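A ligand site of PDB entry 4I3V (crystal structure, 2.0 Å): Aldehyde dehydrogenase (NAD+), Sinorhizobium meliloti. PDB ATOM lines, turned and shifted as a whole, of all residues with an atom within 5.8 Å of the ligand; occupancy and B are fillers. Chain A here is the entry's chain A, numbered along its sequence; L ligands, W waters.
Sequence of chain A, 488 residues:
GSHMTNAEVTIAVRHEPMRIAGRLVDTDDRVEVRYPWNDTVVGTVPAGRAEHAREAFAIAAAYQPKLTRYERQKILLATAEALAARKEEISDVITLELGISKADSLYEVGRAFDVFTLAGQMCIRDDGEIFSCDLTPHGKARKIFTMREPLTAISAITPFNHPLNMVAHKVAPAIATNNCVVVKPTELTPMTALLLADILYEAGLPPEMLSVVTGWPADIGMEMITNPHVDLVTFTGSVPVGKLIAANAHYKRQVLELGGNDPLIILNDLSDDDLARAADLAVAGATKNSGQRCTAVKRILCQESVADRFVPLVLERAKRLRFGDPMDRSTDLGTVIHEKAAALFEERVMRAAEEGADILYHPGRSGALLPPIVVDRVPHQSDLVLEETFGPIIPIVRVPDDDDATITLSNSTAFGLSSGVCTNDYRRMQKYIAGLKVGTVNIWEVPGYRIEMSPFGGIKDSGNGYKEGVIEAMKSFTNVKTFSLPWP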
ATOM      1  N   ILE A 157     -33.470 -22.370 -13.140  1.00  0.00           N
ATOM      2  CA  ILE A 157     -32.091 -22.820 -13.383  1.00  0.00           C
ATOM      3  C   ILE A 157     -31.138 -21.627 -13.200  1.00  0.00           C
ATOM      4  O   ILE A 157     -31.284 -20.602 -13.857  1.00  0.00           O
ATOM      5  CB  ILE A 157     -31.924 -23.400 -14.799  1.00  0.00           C
ATOM      6  CG1 ILE A 157     -32.890 -24.578 -15.021  1.00  0.00           C
ATOM      7  CG2 ILE A 157     -30.497 -23.844 -15.026  1.00  0.00           C
ATOM      8  CD1 ILE A 157     -33.047 -25.003 -16.480  1.00  0.00           C
ATOM      9  N   THR A 158     -30.184 -21.757 -12.286  1.00  0.00           N
ATOM     10  CA  THR A 158     -29.352 -20.620 -11.903  1.00  0.00           C
ATOM     11  C   THR A 158     -27.851 -20.870 -12.106  1.00  0.00           C
ATOM     12  O   THR A 158     -27.388 -22.016 -12.024  1.00  0.00           O
ATOM     13  CB  THR A 158     -29.600 -20.228 -10.441  1.00  0.00           C
ATOM     14  OG1 THR A 158     -29.419 -21.392  -9.603  1.00  0.00           O
ATOM     15  CG2 THR A 158     -31.027 -19.682 -10.269  1.00  0.00           C
ATOM     16  N   PRO A 159     -27.083 -19.791 -12.350  1.00  0.00           N
ATOM     17  CA  PRO A 159     -25.648 -19.864 -12.624  1.00  0.00           C
ATOM     18  C   PRO A 159     -24.818 -19.700 -11.334  1.00  0.00           C
ATOM     19  O   PRO A 159     -25.387 -19.580 -10.241  1.00  0.00           O
ATOM     20  CB  PRO A 159     -25.432 -18.674 -13.553  1.00  0.00           C
ATOM     21  CG  PRO A 159     -26.383 -17.624 -12.992  1.00  0.00           C
ATOM     22  CD  PRO A 159     -27.559 -18.397 -12.384  1.00  0.00           C
ATOM     23  N   PHE A 160     -23.487 -19.673 -11.461  1.00  0.00           N
ATOM     24  CA  PHE A 160     -22.615 -19.689 -10.279  1.00  0.00           C
ATOM     25  C   PHE A 160     -22.422 -18.285  -9.730  1.00  0.00           C
ATOM     26  O   PHE A 160     -21.971 -18.081  -8.591  1.00  0.00           O
ATOM     27  CB  PHE A 160     -21.255 -20.310 -10.627  1.00  0.00           C
ATOM     28  CG  PHE A 160     -20.476 -19.554 -11.669  1.00  0.00           C
ATOM     29  CD1 PHE A 160     -19.729 -18.435 -11.338  1.00  0.00           C
ATOM     30  CD2 PHE A 160     -20.461 -19.991 -13.002  1.00  0.00           C
ATOM     31  CE1 PHE A 160     -18.992 -17.754 -12.295  1.00  0.00           C
ATOM     32  CE2 PHE A 160     -19.718 -19.317 -13.969  1.00  0.00           C
ATOM     33  CZ  PHE A 160     -18.988 -18.185 -13.609  1.00  0.00           C
ATOM     34  N   ASN A 161     -22.788 -17.339 -10.577  1.00  0.00           N
ATOM     35  CA  ASN A 161     -22.641 -15.908 -10.351  1.00  0.00           C
ATOM     36  C   ASN A 161     -22.995 -15.345  -8.971  1.00  0.00           C
ATOM     37  O   ASN A 161     -22.197 -14.642  -8.327  1.00  0.00           O
ATOM     38  CB  ASN A 161     -23.551 -15.224 -11.382  1.00  0.00           C
ATOM     39  CG  ASN A 161     -22.926 -14.031 -11.956  1.00  0.00           C
ATOM     40  OD1 ASN A 161     -21.732 -14.044 -12.241  1.00  0.00           O
ATOM     41  ND2 ASN A 161     -23.701 -12.971 -12.106  1.00  0.00           N
ATOM     42  N   LYS A 184     -32.786 -25.880  -9.905  1.00  0.00           N
ATOM     43  CA  LYS A 184     -31.527 -26.593 -10.122  1.00  0.00           C
ATOM     44  C   LYS A 184     -30.364 -25.606 -10.255  1.00  0.00           C
ATOM     45  O   LYS A 184     -30.100 -25.093 -11.332  1.00  0.00           O
ATOM     46  CB  LYS A 184     -31.588 -27.468 -11.382  1.00  0.00           C
ATOM     47  CG  LYS A 184     -30.343 -28.358 -11.549  1.00  0.00           C
ATOM     48  CD  LYS A 184     -29.911 -28.448 -13.014  1.00  0.00           C
ATOM     49  CE  LYS A 184     -29.279 -27.146 -13.496  1.00  0.00           C
ATOM     50  NZ  LYS A 184     -28.067 -26.779 -12.679  1.00  0.00           N
ATOM     51  N   PRO A 185     -29.669 -25.331  -9.150  1.00  0.00           N
ATOM     52  CA  PRO A 185     -28.526 -24.414  -9.138  1.00  0.00           C
ATOM     53  C   PRO A 185     -27.380 -25.069  -9.871  1.00  0.00           C
ATOM     54  O   PRO A 185     -27.418 -26.284 -10.095  1.00  0.00           O
ATOM     55  CB  PRO A 185     -28.193 -24.311  -7.658  1.00  0.00           C
ATOM     56  CG  PRO A 185     -28.590 -25.684  -7.113  1.00  0.00           C
ATOM     57  CD  PRO A 185     -29.869 -25.986  -7.843  1.00  0.00           C
ATOM     58  N   THR A 186     -26.367 -24.285 -10.237  1.00  0.00           N
ATOM     59  CA  THR A 186     -25.221 -24.855 -10.923  1.00  0.00           C
ATOM     60  C   THR A 186     -24.541 -25.877 -10.029  1.00  0.00           C
ATOM     61  O   THR A 186     -24.516 -25.744  -8.804  1.00  0.00           O
ATOM     62  CB  THR A 186     -24.208 -23.765 -11.334  1.00  0.00           C
ATOM     63  OG1 THR A 186     -23.038 -24.397 -11.871  1.00  0.00           O
ATOM     64  CG2 THR A 186     -23.802 -22.921 -10.127  1.00  0.00           C
ATOM     65  N   GLU A 187     -23.984 -26.919 -10.629  1.00  0.00           N
ATOM     66  CA  GLU A 187     -23.234 -27.905  -9.862  1.00  0.00           C
ATOM     67  C   GLU A 187     -21.987 -27.292  -9.241  1.00  0.00           C
ATOM     68  O   GLU A 187     -21.433 -27.857  -8.315  1.00  0.00           O
ATOM     69  CB  GLU A 187     -22.861 -29.119 -10.740  1.00  0.00           C
ATOM     70  CG  GLU A 187     -21.810 -28.857 -11.803  1.00  0.00           C
ATOM     71  CD  GLU A 187     -22.364 -28.174 -13.049  1.00  0.00           C
ATOM     72  OE1 GLU A 187     -23.578 -27.861 -13.094  1.00  0.00           O
ATOM     73  OE2 GLU A 187     -21.573 -27.949 -13.996  1.00  0.00           O
ATOM     74  N   LEU A 188     -21.560 -26.137  -9.747  1.00  0.00           N
ATOM     75  CA  LEU A 188     -20.386 -25.439  -9.213  1.00  0.00           C
ATOM     76  C   LEU A 188     -20.620 -24.733  -7.880  1.00  0.00           C
ATOM     77  O   LEU A 188     -19.674 -24.553  -7.098  1.00  0.00           O
ATOM     78  CB  LEU A 188     -19.872 -24.398 -10.218  1.00  0.00           C
ATOM     79  CG  LEU A 188     -19.301 -24.868 -11.547  1.00  0.00           C
ATOM     80  CD1 LEU A 188     -19.011 -23.674 -12.423  1.00  0.00           C
ATOM     81  CD2 LEU A 188     -18.047 -25.719 -11.334  1.00  0.00           C
ATOM     82  N   PRO A 217     -25.513 -31.531 -15.541  1.00  0.00           N
ATOM     83  CA  PRO A 217     -26.498 -31.103 -16.544  1.00  0.00           C
ATOM     84  C   PRO A 217     -26.935 -32.234 -17.494  1.00  0.00           C
ATOM     85  O   PRO A 217     -28.100 -32.262 -17.898  1.00  0.00           O
ATOM     86  CB  PRO A 217     -25.763 -30.000 -17.316  1.00  0.00           C
ATOM     87  CG  PRO A 217     -24.698 -29.533 -16.401  1.00  0.00           C
ATOM     88  CD  PRO A 217     -24.286 -30.714 -15.580  1.00  0.00           C
ATOM     89  N   ALA A 218     -26.038 -33.160 -17.816  1.00  0.00           N
ATOM     90  CA  ALA A 218     -26.350 -34.212 -18.793  1.00  0.00           C
ATOM     91  C   ALA A 218     -27.351 -35.286 -18.347  1.00  0.00           C
ATOM     92  O   ALA A 218     -27.705 -36.162 -19.135  1.00  0.00           O
ATOM     93  CB  ALA A 218     -25.059 -34.884 -19.274  1.00  0.00           C
ATOM     94  N   GLY A 221     -30.694 -31.839 -16.219  1.00  0.00           N
ATOM     95  CA  GLY A 221     -31.014 -30.554 -16.831  1.00  0.00           C
ATOM     96  C   GLY A 221     -32.159 -30.609 -17.830  1.00  0.00           C
ATOM     97  O   GLY A 221     -32.967 -29.681 -17.904  1.00  0.00           O
ATOM     98  N   MET A 222     -32.222 -31.684 -18.593  1.00  0.00           N
ATOM     99  CA  MET A 222     -33.261 -31.839 -19.620  1.00  0.00           C
ATOM    100  C   MET A 222     -34.657 -31.962 -19.003  1.00  0.00           C
ATOM    101  O   MET A 222     -35.645 -31.431 -19.532  1.00  0.00           O
ATOM    102  CB  MET A 222     -32.971 -33.047 -20.495  1.00  0.00           C
ATOM    103  CG  MET A 222     -33.896 -33.191 -21.703  1.00  0.00           C
ATOM    104  SD  MET A 222     -33.899 -31.745 -22.789  1.00  0.00           S
ATOM    105  CE  MET A 222     -32.136 -31.495 -23.098  1.00  0.00           C
ATOM    106  N   ILE A 225     -36.274 -28.774 -18.154  1.00  0.00           N
ATOM    107  CA  ILE A 225     -36.690 -28.017 -19.328  1.00  0.00           C
ATOM    108  C   ILE A 225     -37.936 -28.627 -19.970  1.00  0.00           C
ATOM    109  O   ILE A 225     -38.737 -27.933 -20.587  1.00  0.00           O
ATOM    110  CB  ILE A 225     -35.560 -28.030 -20.387  1.00  0.00           C
ATOM    111  CG1 ILE A 225     -34.303 -27.386 -19.811  1.00  0.00           C
ATOM    112  CG2 ILE A 225     -35.974 -27.325 -21.679  1.00  0.00           C
ATOM    113  CD1 ILE A 225     -33.087 -27.569 -20.693  1.00  0.00           C
ATOM    114  N   PHE A 235     -34.499 -18.840 -16.382  1.00  0.00           N
ATOM    115  CA  PHE A 235     -33.096 -19.233 -16.514  1.00  0.00           C
ATOM    116  C   PHE A 235     -32.168 -18.013 -16.573  1.00  0.00           C
ATOM    117  O   PHE A 235     -32.477 -17.018 -17.223  1.00  0.00           O
ATOM    118  CB  PHE A 235     -32.917 -20.061 -17.793  1.00  0.00           C
ATOM    119  CG  PHE A 235     -31.478 -20.262 -18.217  1.00  0.00           C
ATOM    120  CD1 PHE A 235     -30.703 -21.275 -17.631  1.00  0.00           C
ATOM    121  CD2 PHE A 235     -30.913 -19.493 -19.210  1.00  0.00           C
ATOM    122  CE1 PHE A 235     -29.396 -21.485 -18.025  1.00  0.00           C
ATOM    123  CE2 PHE A 235     -29.590 -19.688 -19.613  1.00  0.00           C
ATOM    124  CZ  PHE A 235     -28.830 -20.693 -19.023  1.00  0.00           C
ATOM    125  N   THR A 236     -31.034 -18.102 -15.877  1.00  0.00           N
ATOM    126  CA  THR A 236     -29.958 -17.113 -15.999  1.00  0.00           C
ATOM    127  C   THR A 236     -28.663 -17.864 -16.254  1.00  0.00           C
ATOM    128  O   THR A 236     -28.358 -18.844 -15.578  1.00  0.00           O
ATOM    129  CB  THR A 236     -29.848 -16.241 -14.725  1.00  0.00           C
ATOM    130  OG1 THR A 236     -31.099 -15.584 -14.473  1.00  0.00           O
ATOM    131  CG2 THR A 236     -28.758 -15.195 -14.860  1.00  0.00           C
ATOM    132  N   GLY A 237     -27.898 -17.419 -17.248  1.00  0.00           N
ATOM    133  CA  GLY A 237     -26.702 -18.120 -17.661  1.00  0.00           C
ATOM    134  C   GLY A 237     -26.205 -17.689 -19.030  1.00  0.00           C
ATOM    135  O   GLY A 237     -26.404 -16.549 -19.451  1.00  0.00           O
ATOM    136  N   SER A 238     -25.560 -18.615 -19.738  1.00  0.00           N
ATOM    137  CA  SER A 238     -24.900 -18.277 -20.996  1.00  0.00           C
ATOM    138  C   SER A 238     -25.832 -18.413 -22.194  1.00  0.00           C
ATOM    139  O   SER A 238     -26.849 -19.135 -22.130  1.00  0.00           O
ATOM    140  CB  SER A 238     -23.657 -19.166 -21.223  1.00  0.00           C
ATOM    141  OG  SER A 238     -23.995 -20.526 -21.406  1.00  0.00           O
ATOM    142  N   VAL A 239     -25.472 -17.737 -23.278  1.00  0.00           N
ATOM    143  CA  VAL A 239     -26.204 -17.797 -24.532  1.00  0.00           C
ATOM    144  C   VAL A 239     -26.340 -19.226 -25.057  1.00  0.00           C
ATOM    145  O   VAL A 239     -27.449 -19.674 -25.357  1.00  0.00           O
ATOM    146  CB  VAL A 239     -25.550 -16.920 -25.635  1.00  0.00           C
ATOM    147  CG1 VAL A 239     -26.276 -17.121 -26.959  1.00  0.00           C
ATOM    148  CG2 VAL A 239     -25.555 -15.444 -25.233  1.00  0.00           C
ATOM    149  N   VAL A 241     -26.309 -22.089 -23.615  1.00  0.00           N
ATOM    150  CA  VAL A 241     -27.223 -22.899 -22.815  1.00  0.00           C
ATOM    151  C   VAL A 241     -28.628 -22.338 -22.944  1.00  0.00           C
ATOM    152  O   VAL A 241     -29.600 -23.090 -23.016  1.00  0.00           O
ATOM    153  CB  VAL A 241     -26.788 -22.975 -21.327  1.00  0.00           C
ATOM    154  CG1 VAL A 241     -27.868 -23.676 -20.494  1.00  0.00           C
ATOM    155  CG2 VAL A 241     -25.438 -23.690 -21.200  1.00  0.00           C
ATOM    156  N   GLY A 242     -28.727 -21.016 -23.000  1.00  0.00           N
ATOM    157  CA  GLY A 242     -30.002 -20.384 -23.226  1.00  0.00           C
ATOM    158  C   GLY A 242     -30.672 -20.938 -24.476  1.00  0.00           C
ATOM    159  O   GLY A 242     -31.872 -21.224 -24.500  1.00  0.00           O
ATOM    160  N   LEU A 244     -30.103 -23.829 -25.880  1.00  0.00           N
ATOM    161  CA  LEU A 244     -30.503 -25.202 -25.631  1.00  0.00           C
ATOM    162  C   LEU A 244     -31.862 -25.230 -24.932  1.00  0.00           C
ATOM    163  O   LEU A 244     -32.708 -26.074 -25.231  1.00  0.00           O
ATOM    164  CB  LEU A 244     -29.455 -25.913 -24.777  1.00  0.00           C
ATOM    165  CG  LEU A 244     -29.692 -27.375 -24.439  1.00  0.00           C
ATOM    166  CD1 LEU A 244     -28.363 -28.140 -24.408  1.00  0.00           C
ATOM    167  CD2 LEU A 244     -30.399 -27.518 -23.107  1.00  0.00           C
ATOM    168  N   ILE A 245     -32.071 -24.306 -23.996  1.00  0.00           N
ATOM    169  CA  ILE A 245     -33.343 -24.260 -23.276  1.00  0.00           C
ATOM    170  C   ILE A 245     -34.496 -23.964 -24.231  1.00  0.00           C
ATOM    171  O   ILE A 245     -35.449 -24.724 -24.295  1.00  0.00           O
ATOM    172  CB  ILE A 245     -33.295 -23.278 -22.112  1.00  0.00           C
ATOM    173  CG1 ILE A 245     -32.432 -23.883 -20.991  1.00  0.00           C
ATOM    174  CG2 ILE A 245     -34.723 -22.987 -21.599  1.00  0.00           C
ATOM    175  CD1 ILE A 245     -31.856 -22.866 -20.066  1.00  0.00           C
ATOM    176  N   PHE A 390     -15.309 -12.647 -17.968  1.00  0.00           N
ATOM    177  CA  PHE A 390     -16.113 -12.633 -16.752  1.00  0.00           C
ATOM    178  C   PHE A 390     -15.190 -12.581 -15.547  1.00  0.00           C
ATOM    179  O   PHE A 390     -15.271 -13.430 -14.661  1.00  0.00           O
ATOM    180  CB  PHE A 390     -16.938 -13.929 -16.740  1.00  0.00           C
ATOM    181  CG  PHE A 390     -18.292 -13.799 -16.112  1.00  0.00           C
ATOM    182  CD1 PHE A 390     -19.156 -12.796 -16.502  1.00  0.00           C
ATOM    183  CD2 PHE A 390     -18.714 -14.721 -15.165  1.00  0.00           C
ATOM    184  CE1 PHE A 390     -20.424 -12.690 -15.940  1.00  0.00           C
ATOM    185  CE2 PHE A 390     -19.968 -14.626 -14.586  1.00  0.00           C
ATOM    186  CZ  PHE A 390     -20.827 -13.602 -14.967  1.00  0.00           C
HETATM  187  P1  LIG L   1     -24.122 -21.729 -17.812  1.00  0.00           P
HETATM  188  O1  LIG L   1     -23.084 -22.669 -18.318  1.00  0.00           O
HETATM  189  O2  LIG L   1     -25.026 -21.342 -18.910  1.00  0.00           O
HETATM  190  O3  LIG L   1     -24.870 -22.399 -16.576  1.00  0.00           O
HETATM  191  C1  LIG L   1     -26.153 -21.931 -16.099  1.00  0.00           C
HETATM  192  C2  LIG L   1     -27.054 -22.945 -15.593  1.00  0.00           C
HETATM  193  O4  LIG L   1     -27.443 -23.782 -16.648  1.00  0.00           O
HETATM  194  C3  LIG L   1     -26.374 -23.819 -14.600  1.00  0.00           C
HETATM  195  O5  LIG L   1     -27.321 -24.248 -13.654  1.00  0.00           O
HETATM  196  C4  LIG L   1     -25.970 -24.911 -15.368  1.00  0.00           C
HETATM  197  O6  LIG L   1     -25.721 -26.035 -14.575  1.00  0.00           O
HETATM  198  C5  LIG L   1     -27.152 -25.105 -16.262  1.00  0.00           C
HETATM  199  N1  LIG L   1     -26.944 -25.919 -17.474  1.00  0.00           N
HETATM  200  C6  LIG L   1     -25.807 -26.004 -18.173  1.00  0.00           C
HETATM  201  N2  LIG L   1     -25.969 -26.841 -19.220  1.00  0.00           N
HETATM  202  C7  LIG L   1     -27.232 -27.296 -19.172  1.00  0.00           C
HETATM  203  C8  LIG L   1     -27.958 -28.178 -19.955  1.00  0.00           C
HETATM  204  N3  LIG L   1     -27.371 -28.792 -21.091  1.00  0.00           N
HETATM  205  N4  LIG L   1     -29.244 -28.437 -19.632  1.00  0.00           N
HETATM  206  C9  LIG L   1     -29.820 -27.860 -18.570  1.00  0.00           C
HETATM  207  N5  LIG L   1     -29.141 -27.014 -17.800  1.00  0.00           N
HETATM  208  C10 LIG L   1     -27.857 -26.714 -18.066  1.00  0.00           C
HETATM  209  O7  LIG L   1     -23.529 -20.358 -17.309  1.00  0.00           O
HETATM  210  P2  LIG L   1     -22.626 -20.186 -16.047  1.00  0.00           P
HETATM  211  O8  LIG L   1     -21.285 -20.763 -16.428  1.00  0.00           O
HETATM  212  O9  LIG L   1     -22.503 -18.696 -15.771  1.00  0.00           O
HETATM  213  O10 LIG L   1     -23.220 -20.900 -14.750  1.00  0.00           O
HETATM  214  O   HOH W   1     -26.150 -28.758 -13.056  1.00  0.00           O
HETATM  215  O   HOH W   2     -23.196 -26.347 -15.182  1.00  0.00           O
HETATM  216  O   HOH W   3     -22.316 -16.856 -13.520  1.00  0.00           O
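The side-chain hydroxyl of Ser 238 sits at hydrogen-bond distance from an oxygen (O2) of the ligand.
OE1 of Glu 187 lies within hydrogen-bond range of O6 of the ligand.
N of Ser 238 lies within hydrogen-bond range of O2 of the ligand (2.9 Å).
The backbone carbonyl oxygen (O) of Thr 158 sits at hydrogen-bond distance from an oxygen (O5) of the ligand, at 2.8 Å.
The side-chain amino group (NZ) of Lys 184 sits at hydrogen-bond distance from an oxygen (O5) of the ligand.
Water W2 bridges OE2 of Glu 187 (2.6 Å) and O6 of the ligand (2.6 Å).
Water W3 lies within hydrogen-bond range of O9 of the ligand (2.9 Å) and N of Asn 161 (3.0 Å).
Water W1 lies within hydrogen-bond range of the side-chain carboxylate of Glu 187, the side-chain amino group of Lys 184 and an oxygen (O6) of the ligand.
N of Thr 186 is in hydrogen-bond range of O of Thr 158, 3.1 Å away.
N of Thr 158 is in hydrogen-bond range of O of Lys 184, 3.5 Å away.
OG1 of Thr 186 lies close to N of Leu 188 (3.1 Å).
N of Thr 236 lies within hydrogen-bond range of O of Ile 157, at 3.2 Å.
Residues that only touch the ligand: Ile 157 (3.5 Å), Pro 159 (3.4 Å), Phe 160 (3.3 Å), Pro 185 (3.9 Å), Thr 186 (3.5 Å), Pro 217 (3.6 Å), Gly 221 (3.4 Å), Ile 225 (3.9 Å), Phe 235 (3.3 Å), Thr 236 (3.8 Å), Gly 237 (3.8 Å), Val 241 (3.3 Å) and Leu 244 (3.5 Å).
Hydrophobic or aromatic side chains that line the ligand: Ile 157, Pro 159, Phe 160, Pro 217, Ile 225, Phe 235, Val 241 and Leu 244.
The nearest printed residue that does not touch the ligand is Met 222 (4.5 Å).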
